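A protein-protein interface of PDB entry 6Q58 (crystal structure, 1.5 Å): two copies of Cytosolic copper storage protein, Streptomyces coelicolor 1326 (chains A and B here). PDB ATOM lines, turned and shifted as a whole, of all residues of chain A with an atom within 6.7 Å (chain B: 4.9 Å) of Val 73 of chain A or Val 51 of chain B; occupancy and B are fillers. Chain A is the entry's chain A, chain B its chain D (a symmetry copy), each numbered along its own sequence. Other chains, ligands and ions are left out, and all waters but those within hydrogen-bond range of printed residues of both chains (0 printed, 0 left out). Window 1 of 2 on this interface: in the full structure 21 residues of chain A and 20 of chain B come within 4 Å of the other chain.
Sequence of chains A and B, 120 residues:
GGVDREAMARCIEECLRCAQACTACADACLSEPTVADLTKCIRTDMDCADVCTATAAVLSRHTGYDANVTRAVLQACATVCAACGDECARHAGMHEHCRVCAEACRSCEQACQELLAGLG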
ATOM      1  N   VAL A  51     -13.614 -15.671 -16.262  1.00  0.00           N
ATOM      2  CA  VAL A  51     -12.712 -15.637 -15.137  1.00  0.00           C
ATOM      3  C   VAL A  51     -12.952 -16.820 -14.204  1.00  0.00           C
ATOM      4  O   VAL A  51     -12.015 -17.394 -13.667  1.00  0.00           O
ATOM      5  CB  VAL A  51     -12.755 -14.271 -14.425  1.00  0.00           C
ATOM      6  CG1 VAL A  51     -11.926 -14.269 -13.191  1.00  0.00           C
ATOM      7  CG2 VAL A  51     -12.251 -13.200 -15.401  1.00  0.00           C
ATOM      8  N   ALA A  54     -11.256 -19.954 -15.707  1.00  0.00           N
ATOM      9  CA  ALA A  54      -9.794 -19.842 -15.513  1.00  0.00           C
ATOM     10  C   ALA A  54      -9.407 -20.082 -14.077  1.00  0.00           C
ATOM     11  O   ALA A  54      -8.431 -20.788 -13.762  1.00  0.00           O
ATOM     12  CB  ALA A  54      -9.296 -18.497 -15.951  1.00  0.00           C
ATOM     13  N   THR A  55     -10.183 -19.499 -13.146  1.00  0.00           N
ATOM     14  CA  THR A  55      -9.886 -19.643 -11.734  1.00  0.00           C
ATOM     15  C   THR A  55     -10.014 -21.103 -11.291  1.00  0.00           C
ATOM     16  O   THR A  55      -9.172 -21.614 -10.557  1.00  0.00           O
ATOM     17  CB  THR A  55     -10.804 -18.710 -10.879  1.00  0.00           C
ATOM     18  OG1 THR A  55     -10.537 -17.358 -11.273  1.00  0.00           O
ATOM     19  CG2 THR A  55     -10.582 -18.884  -9.415  1.00  0.00           C
ATOM     20  N   ALA A  56     -11.076 -21.791 -11.732  1.00  0.00           N
ATOM     21  CA  ALA A  56     -11.253 -23.212 -11.391  1.00  0.00           C
ATOM     22  C   ALA A  56     -10.009 -24.018 -11.894  1.00  0.00           C
ATOM     23  O   ALA A  56      -9.543 -24.890 -11.219  1.00  0.00           O
ATOM     24  CB  ALA A  56     -12.533 -23.763 -11.984  1.00  0.00           C
ATOM     25  N   VAL A  58      -6.818 -22.876 -12.494  1.00  0.00           N
ATOM     26  CA  VAL A  58      -5.655 -22.521 -11.684  1.00  0.00           C
ATOM     27  C   VAL A  58      -5.699 -23.199 -10.309  1.00  0.00           C
ATOM     28  O   VAL A  58      -4.709 -23.744  -9.824  1.00  0.00           O
ATOM     29  CB  VAL A  58      -5.504 -20.996 -11.554  1.00  0.00           C
ATOM     30  CG1 VAL A  58      -4.426 -20.620 -10.532  1.00  0.00           C
ATOM     31  CG2 VAL A  58      -5.197 -20.388 -12.928  1.00  0.00           C
ATOM     32  N   LEU A  59      -6.866 -23.174  -9.661  1.00  0.00           N
ATOM     33  CA  LEU A  59      -7.026 -23.794  -8.359  1.00  0.00           C
ATOM     34  C   LEU A  59      -6.830 -25.309  -8.379  1.00  0.00           C
ATOM     35  O   LEU A  59      -6.468 -25.887  -7.391  1.00  0.00           O
ATOM     36  CB  LEU A  59      -8.378 -23.461  -7.737  1.00  0.00           C
ATOM     37  CG  LEU A  59      -8.574 -22.018  -7.359  1.00  0.00           C
ATOM     38  CD1 LEU A  59     -10.015 -21.859  -6.880  1.00  0.00           C
ATOM     39  CD2 LEU A  59      -7.595 -21.599  -6.259  1.00  0.00           C
ATOM     40  N   ASN A  68       1.342 -16.414  -4.724  1.00  0.00           N
ATOM     41  CA  ASN A  68       1.114 -15.065  -5.265  1.00  0.00           C
ATOM     42  C   ASN A  68       0.256 -15.087  -6.518  1.00  0.00           C
ATOM     43  O   ASN A  68      -0.604 -14.222  -6.739  1.00  0.00           O
ATOM     44  CB  ASN A  68       2.434 -14.323  -5.561  1.00  0.00           C
ATOM     45  CG  ASN A  68       3.336 -14.244  -4.345  1.00  0.00           C
ATOM     46  OD1 ASN A  68       2.856 -14.150  -3.203  1.00  0.00           O
ATOM     47  ND2 ASN A  68       4.631 -14.346  -4.574  1.00  0.00           N
ATOM     48  N   VAL A  69       0.495 -16.102  -7.359  1.00  0.00           N
ATOM     49  CA  VAL A  69      -0.274 -16.242  -8.593  1.00  0.00           C
ATOM     50  C   VAL A  69      -1.707 -16.609  -8.223  1.00  0.00           C
ATOM     51  O   VAL A  69      -2.651 -16.010  -8.735  1.00  0.00           O
ATOM     52  CB  VAL A  69       0.338 -17.333  -9.495  1.00  0.00           C
ATOM     53  CG1 VAL A  69      -0.628 -17.772 -10.614  1.00  0.00           C
ATOM     54  CG2 VAL A  69       1.670 -16.809 -10.047  1.00  0.00           C
ATOM     55  N   THR A  70      -1.850 -17.634  -7.374  1.00  0.00           N
ATOM     56  CA  THR A  70      -3.149 -18.099  -6.981  1.00  0.00           C
ATOM     57  C   THR A  70      -3.968 -16.967  -6.332  1.00  0.00           C
ATOM     58  O   THR A  70      -5.134 -16.781  -6.653  1.00  0.00           O
ATOM     59  CB  THR A  70      -3.015 -19.325  -6.080  1.00  0.00           C
ATOM     60  OG1 THR A  70      -2.372 -20.379  -6.844  1.00  0.00           O
ATOM     61  CG2 THR A  70      -4.391 -19.835  -5.634  1.00  0.00           C
ATOM     62  N   ARG A  71      -3.359 -16.197  -5.444  1.00  0.00           N
ATOM     63  CA  ARG A  71      -4.049 -15.062  -4.820  1.00  0.00           C
ATOM     64  C   ARG A  71      -4.476 -14.015  -5.825  1.00  0.00           C
ATOM     65  O   ARG A  71      -5.553 -13.487  -5.734  1.00  0.00           O
ATOM     66  CB  ARG A  71      -3.163 -14.393  -3.754  1.00  0.00           C
ATOM     67  CG  ARG A  71      -2.966 -15.206  -2.477  1.00  0.00           C
ATOM     68  CD  ARG A  71      -2.285 -14.340  -1.411  1.00  0.00           C
ATOM     69  NE  ARG A  71      -3.185 -13.310  -0.900  1.00  0.00           N
ATOM     70  CZ  ARG A  71      -4.095 -13.493   0.066  1.00  0.00           C
ATOM     71  NH1 ARG A  71      -4.250 -14.686   0.667  1.00  0.00           N
ATOM     72  NH2 ARG A  71      -4.851 -12.464   0.441  1.00  0.00           N
ATOM     73  N   ALA A  72      -3.630 -13.685  -6.790  1.00  0.00           N
ATOM     74  CA  ALA A  72      -3.990 -12.679  -7.794  1.00  0.00           C
ATOM     75  C   ALA A  72      -5.180 -13.127  -8.645  1.00  0.00           C
ATOM     76  O   ALA A  72      -6.063 -12.316  -8.959  1.00  0.00           O
ATOM     77  CB  ALA A  72      -2.796 -12.322  -8.664  1.00  0.00           C
ATOM     78  N   VAL A  73      -5.220 -14.414  -8.984  1.00  0.00           N
ATOM     79  CA  VAL A  73      -6.325 -14.939  -9.771  1.00  0.00           C
ATOM     80  C   VAL A  73      -7.634 -14.944  -8.905  1.00  0.00           C
ATOM     81  O   VAL A  73      -8.698 -14.565  -9.383  1.00  0.00           O
ATOM     82  CB  VAL A  73      -5.992 -16.337 -10.321  1.00  0.00           C
ATOM     83  CG1 VAL A  73      -7.258 -17.017 -10.947  1.00  0.00           C
ATOM     84  CG2 VAL A  73      -4.832 -16.218 -11.295  1.00  0.00           C
ATOM     85  N   LEU A  74      -7.531 -15.376  -7.648  1.00  0.00           N
ATOM     86  CA  LEU A  74      -8.664 -15.332  -6.739  1.00  0.00           C
ATOM     87  C   LEU A  74      -9.194 -13.913  -6.532  1.00  0.00           C
ATOM     88  O   LEU A  74     -10.409 -13.705  -6.468  1.00  0.00           O
ATOM     89  CB  LEU A  74      -8.296 -15.936  -5.399  1.00  0.00           C
ATOM     90  CG  LEU A  74      -8.244 -17.457  -5.364  1.00  0.00           C
ATOM     91  CD1 LEU A  74      -7.511 -17.905  -4.114  1.00  0.00           C
ATOM     92  CD2 LEU A  74      -9.707 -18.025  -5.470  1.00  0.00           C
ATOM     93  N   GLN A  75      -8.311 -12.938  -6.426  1.00  0.00           N
ATOM     94  CA  GLN A  75      -8.739 -11.535  -6.289  1.00  0.00           C
ATOM     95  C   GLN A  75      -9.518 -11.098  -7.514  1.00  0.00           C
ATOM     96  O   GLN A  75     -10.560 -10.445  -7.409  1.00  0.00           O
ATOM     97  CB  GLN A  75      -7.551 -10.599  -6.016  1.00  0.00           C
ATOM     98  CG  GLN A  75      -8.029  -9.167  -5.769  1.00  0.00           C
ATOM     99  CD  GLN A  75      -8.965  -9.126  -4.572  1.00  0.00           C
ATOM    100  OE1 GLN A  75      -8.544  -9.488  -3.479  1.00  0.00           O
ATOM    101  NE2 GLN A  75     -10.240  -8.744  -4.772  1.00  0.00           N
ATOM    102  N   ALA A  76      -9.031 -11.453  -8.708  1.00  0.00           N
ATOM    103  CA  ALA A  76      -9.727 -11.124  -9.933  1.00  0.00           C
ATOM    104  C   ALA A  76     -11.121 -11.787  -9.955  1.00  0.00           C
ATOM    105  O   ALA A  76     -12.104 -11.142 -10.304  1.00  0.00           O
ATOM    106  CB  ALA A  76      -8.919 -11.540 -11.139  1.00  0.00           C
ATOM    107  N   CYS A  77     -11.178 -13.056  -9.562  1.00  0.00           N
ATOM    108  CA  CYS A  77     -12.432 -13.784  -9.561  1.00  0.00           C
ATOM    109  C   CYS A  77     -13.435 -13.161  -8.559  1.00  0.00           C
ATOM    110  O   CYS A  77     -14.613 -12.923  -8.902  1.00  0.00           O
ATOM    111  CB  CYS A  77     -12.218 -15.269  -9.293  1.00  0.00           C
ATOM    112  SG  CYS A  77     -13.611 -16.283  -9.851  1.00  0.00           S
ATOM    113  N   ALA A  78     -12.947 -12.857  -7.369  1.00  0.00           N
ATOM    114  CA  ALA A  78     -13.808 -12.198  -6.360  1.00  0.00           C
ATOM    115  C   ALA A  78     -14.345 -10.862  -6.882  1.00  0.00           C
ATOM    116  O   ALA A  78     -15.550 -10.556  -6.732  1.00  0.00           O
ATOM    117  CB  ALA A  78     -13.069 -12.005  -5.045  1.00  0.00           C
ATOM    118  N   CYS A 112     -14.378 -17.465  -3.008  1.00  0.00           N
ATOM    119  CA  CYS A 112     -13.077 -16.891  -3.388  1.00  0.00           C
ATOM    120  C   CYS A 112     -12.484 -16.057  -2.252  1.00  0.00           C
ATOM    121  O   CYS A 112     -11.313 -16.144  -1.953  1.00  0.00           O
ATOM    122  CB  CYS A 112     -13.205 -16.050  -4.654  1.00  0.00           C
ATOM    123  SG  CYS A 112     -13.508 -16.997  -6.148  1.00  0.00           S
ATOM    124  N   LEU A 116      -8.984 -16.493  -0.240  1.00  0.00           N
ATOM    125  CA  LEU A 116      -8.086 -15.335  -0.075  1.00  0.00           C
ATOM    126  C   LEU A 116      -7.697 -15.081   1.391  1.00  0.00           C
ATOM    127  O   LEU A 116      -6.547 -14.797   1.697  1.00  0.00           O
ATOM    128  CB  LEU A 116      -8.712 -14.055  -0.630  1.00  0.00           C
ATOM    129  CG  LEU A 116      -8.626 -13.853  -2.138  1.00  0.00           C
ATOM    130  CD1 LEU A 116      -9.655 -12.844  -2.594  1.00  0.00           C
ATOM    131  CD2 LEU A 116      -7.218 -13.470  -2.501  1.00  0.00           C
ATOM    132  N   ASP B  47      -1.166 -22.098 -16.342  1.00  0.00           N
ATOM    133  CA  ASP B  47      -1.843 -20.984 -15.667  1.00  0.00           C
ATOM    134  C   ASP B  47      -1.841 -19.709 -16.501  1.00  0.00           C
ATOM    135  O   ASP B  47      -2.851 -18.993 -16.616  1.00  0.00           O
ATOM    136  CB  ASP B  47      -1.187 -20.668 -14.320  1.00  0.00           C
ATOM    137  CG  ASP B  47      -1.452 -21.677 -13.251  1.00  0.00           C
ATOM    138  OD1 ASP B  47      -2.356 -22.515 -13.361  1.00  0.00           O
ATOM    139  OD2 ASP B  47      -0.728 -21.562 -12.233  1.00  0.00           O
ATOM    140  N   CYS B  48      -0.704 -19.393 -17.100  1.00  0.00           N
ATOM    141  CA  CYS B  48      -0.570 -18.195 -17.875  1.00  0.00           C
ATOM    142  C   CYS B  48      -1.486 -18.222 -19.091  1.00  0.00           C
ATOM    143  O   CYS B  48      -2.174 -17.237 -19.384  1.00  0.00           O
ATOM    144  CB  CYS B  48       0.898 -18.010 -18.260  1.00  0.00           C
ATOM    145  SG  CYS B  48       1.245 -16.353 -18.851  1.00  0.00           S
ATOM    146  N   ALA B  49      -1.553 -19.346 -19.798  1.00  0.00           N
ATOM    147  CA  ALA B  49      -2.468 -19.462 -20.930  1.00  0.00           C
ATOM    148  C   ALA B  49      -3.914 -19.260 -20.504  1.00  0.00           C
ATOM    149  O   ALA B  49      -4.632 -18.524 -21.156  1.00  0.00           O
ATOM    150  CB  ALA B  49      -2.309 -20.804 -21.622  1.00  0.00           C
ATOM    151  N   ASP B  50      -4.313 -19.894 -19.414  1.00  0.00           N
ATOM    152  CA  ASP B  50      -5.694 -19.760 -18.944  1.00  0.00           C
ATOM    153  C   ASP B  50      -6.028 -18.309 -18.542  1.00  0.00           C
ATOM    154  O   ASP B  50      -7.122 -17.812 -18.875  1.00  0.00           O
ATOM    155  CB  ASP B  50      -5.964 -20.678 -17.759  1.00  0.00           C
ATOM    156  CG  ASP B  50      -5.991 -22.157 -18.139  1.00  0.00           C
ATOM    157  OD1 ASP B  50      -6.245 -22.495 -19.353  1.00  0.00           O
ATOM    158  OD2 ASP B  50      -5.757 -22.965 -17.225  1.00  0.00           O
ATOM    159  N   VAL B  51      -5.125 -17.650 -17.837  1.00  0.00           N
ATOM    160  CA  VAL B  51      -5.377 -16.287 -17.405  1.00  0.00           C
ATOM    161  C   VAL B  51      -5.332 -15.320 -18.589  1.00  0.00           C
ATOM    162  O   VAL B  51      -6.160 -14.407 -18.696  1.00  0.00           O
ATOM    163  CB  VAL B  51      -4.443 -15.870 -16.271  1.00  0.00           C
ATOM    164  CG1 VAL B  51      -4.662 -14.375 -15.918  1.00  0.00           C
ATOM    165  CG2 VAL B  51      -4.687 -16.737 -15.062  1.00  0.00           C
ATOM    166  N   CYS B  52      -4.385 -15.521 -19.516  1.00  0.00           N
ATOM    167  CA  CYS B  52      -4.308 -14.671 -20.684  1.00  0.00           C
ATOM    168  C   CYS B  52      -5.554 -14.799 -21.566  1.00  0.00           C
ATOM    169  O   CYS B  52      -6.009 -13.823 -22.136  1.00  0.00           O
ATOM    170  CB  CYS B  52      -3.090 -14.982 -21.521  1.00  0.00           C
ATOM    171  SG  CYS B  52      -1.532 -14.328 -20.845  1.00  0.00           S
ATOM    172  N   THR B  53      -6.083 -15.996 -21.700  1.00  0.00           N
ATOM    173  CA  THR B  53      -7.268 -16.259 -22.513  1.00  0.00           C
ATOM    174  C   THR B  53      -8.469 -15.495 -21.916  1.00  0.00           C
ATOM    175  O   THR B  53      -9.215 -14.816 -22.660  1.00  0.00           O
ATOM    176  CB  THR B  53      -7.492 -17.800 -22.539  1.00  0.00           C
ATOM    177  OG1 THR B  53      -6.440 -18.393 -23.298  1.00  0.00           O
ATOM    178  CG2 THR B  53      -8.811 -18.185 -23.151  1.00  0.00           C
ATOM    179  N   ALA B  54      -8.630 -15.595 -20.597  1.00  0.00           N
ATOM    180  CA  ALA B  54      -9.713 -14.875 -19.910  1.00  0.00           C
ATOM    181  C   ALA B  54      -9.524 -13.368 -20.052  1.00  0.00           C
ATOM    182  O   ALA B  54     -10.473 -12.637 -20.330  1.00  0.00           O
ATOM    183  CB  ALA B  54      -9.766 -15.243 -18.462  1.00  0.00           C
ATOM    184  N   THR B  55      -8.282 -12.903 -19.875  1.00  0.00           N
ATOM    185  CA  THR B  55      -7.983 -11.487 -19.934  1.00  0.00           C
ATOM    186  C   THR B  55      -8.261 -10.913 -21.314  1.00  0.00           C
ATOM    187  O   THR B  55      -8.859  -9.834 -21.414  1.00  0.00           O
ATOM    188  CB  THR B  55      -6.521 -11.215 -19.498  1.00  0.00           C
ATOM    189  OG1 THR B  55      -6.319 -11.654 -18.173  1.00  0.00           O
ATOM    190  CG2 THR B  55      -6.203  -9.713 -19.589  1.00  0.00           C
ATOM    191  N   ALA B  76      -4.029  -9.576 -12.356  1.00  0.00           N
ATOM    192  CA  ALA B  76      -3.844 -11.022 -12.341  1.00  0.00           C
ATOM    193  C   ALA B  76      -2.989 -11.467 -13.529  1.00  0.00           C
ATOM    194  O   ALA B  76      -2.064 -12.286 -13.372  1.00  0.00           O
ATOM    195  CB  ALA B  76      -5.176 -11.744 -12.365  1.00  0.00           C
ATOM    196  N   CYS B  77      -3.290 -10.928 -14.700  1.00  0.00           N
ATOM    197  CA  CYS B  77      -2.573 -11.300 -15.918  1.00  0.00           C
ATOM    198  C   CYS B  77      -1.107 -10.874 -15.812  1.00  0.00           C
ATOM    199  O   CYS B  77      -0.196 -11.663 -16.093  1.00  0.00           O
ATOM    200  CB  CYS B  77      -3.261 -10.723 -17.138  1.00  0.00           C
ATOM    201  SG  CYS B  77      -2.772 -11.519 -18.660  1.00  0.00           S
ATOM    202  N   VAL B  80       0.697 -13.287 -13.348  1.00  0.00           N
ATOM    203  CA  VAL B  80       0.943 -14.620 -13.872  1.00  0.00           C
ATOM    204  C   VAL B  80       1.975 -14.601 -15.005  1.00  0.00           C
ATOM    205  O   VAL B  80       2.820 -15.499 -15.091  1.00  0.00           O
ATOM    206  CB  VAL B  80      -0.345 -15.380 -14.329  1.00  0.00           C
ATOM    207  CG1 VAL B  80      -0.939 -14.872 -15.666  1.00  0.00           C
ATOM    208  CG2 VAL B  80      -0.017 -16.880 -14.475  1.00  0.00           C
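Of the 12 printed residues of chain B, 4 touch a printed residue of chain A.
Printed residues of chain B that touch a printed residue of chain A: Asp 47, Asp 50, Val 51 and Ala 76.
Hydrophobic or aromatic side chains of chain B that line the printed part of chain A: Val 51 and Ala 76.
Of the 19 printed residues of chain A, 5 touch a printed residue of chain B.
Printed residues of chain A that touch a printed residue of chain B: Ala 54, Val 58, Ala 72, Val 73 and Ala 76.
Hydrophobic or aromatic side chains of chain A that line the printed part of chain B: Ala 54, Val 58, Val 73 and Ala 76.
Val 73 of chain A touches just one residue of chain B: Val 51 (3.8 Å).
Of the printed residues of chain A, Val 51 of chain B touches Val 73 (3.8 Å).
Printed residues of chain A within 4 Å of Ala 76 of chain B: Ala 72 and Ala 76.
Of the printed residues of chain A, Asp 47 of chain B touches Val 58.
Leu 116 of chain A touches none of the printed residues of chain B.
The nearest printed residue of chain B that does not touch Val 73 of chain A is Ala 76 of chain B (4.3 Å).
The nearest residue of chain A that does not touch Val 51 of chain B is Val 58 of chain A (4.3 Å).
Among the printed residues, merely in contact across the chains: Ala 54 of chain A with Asp 50 of chain B, Val 58 of chain A with Asp 47 of chain B, Ala 72 of chain A with Ala 76 of chain B, Val 73 of chain A with Val 51 of chain B and Ala 76 of chain A with Ala 76 of chain B.
Ala 76 of chain A touches its own counterpart, Ala 76 of chain B.
Positions printed for both chains: 51, 54, 55, 76 and 77.
The backbone carbonyl oxygen (O) of Val 51 of chain B is in hydrogen-bond range of the side-chain hydroxyl (OG1) of Thr 55 of chain B (2.8 Å).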
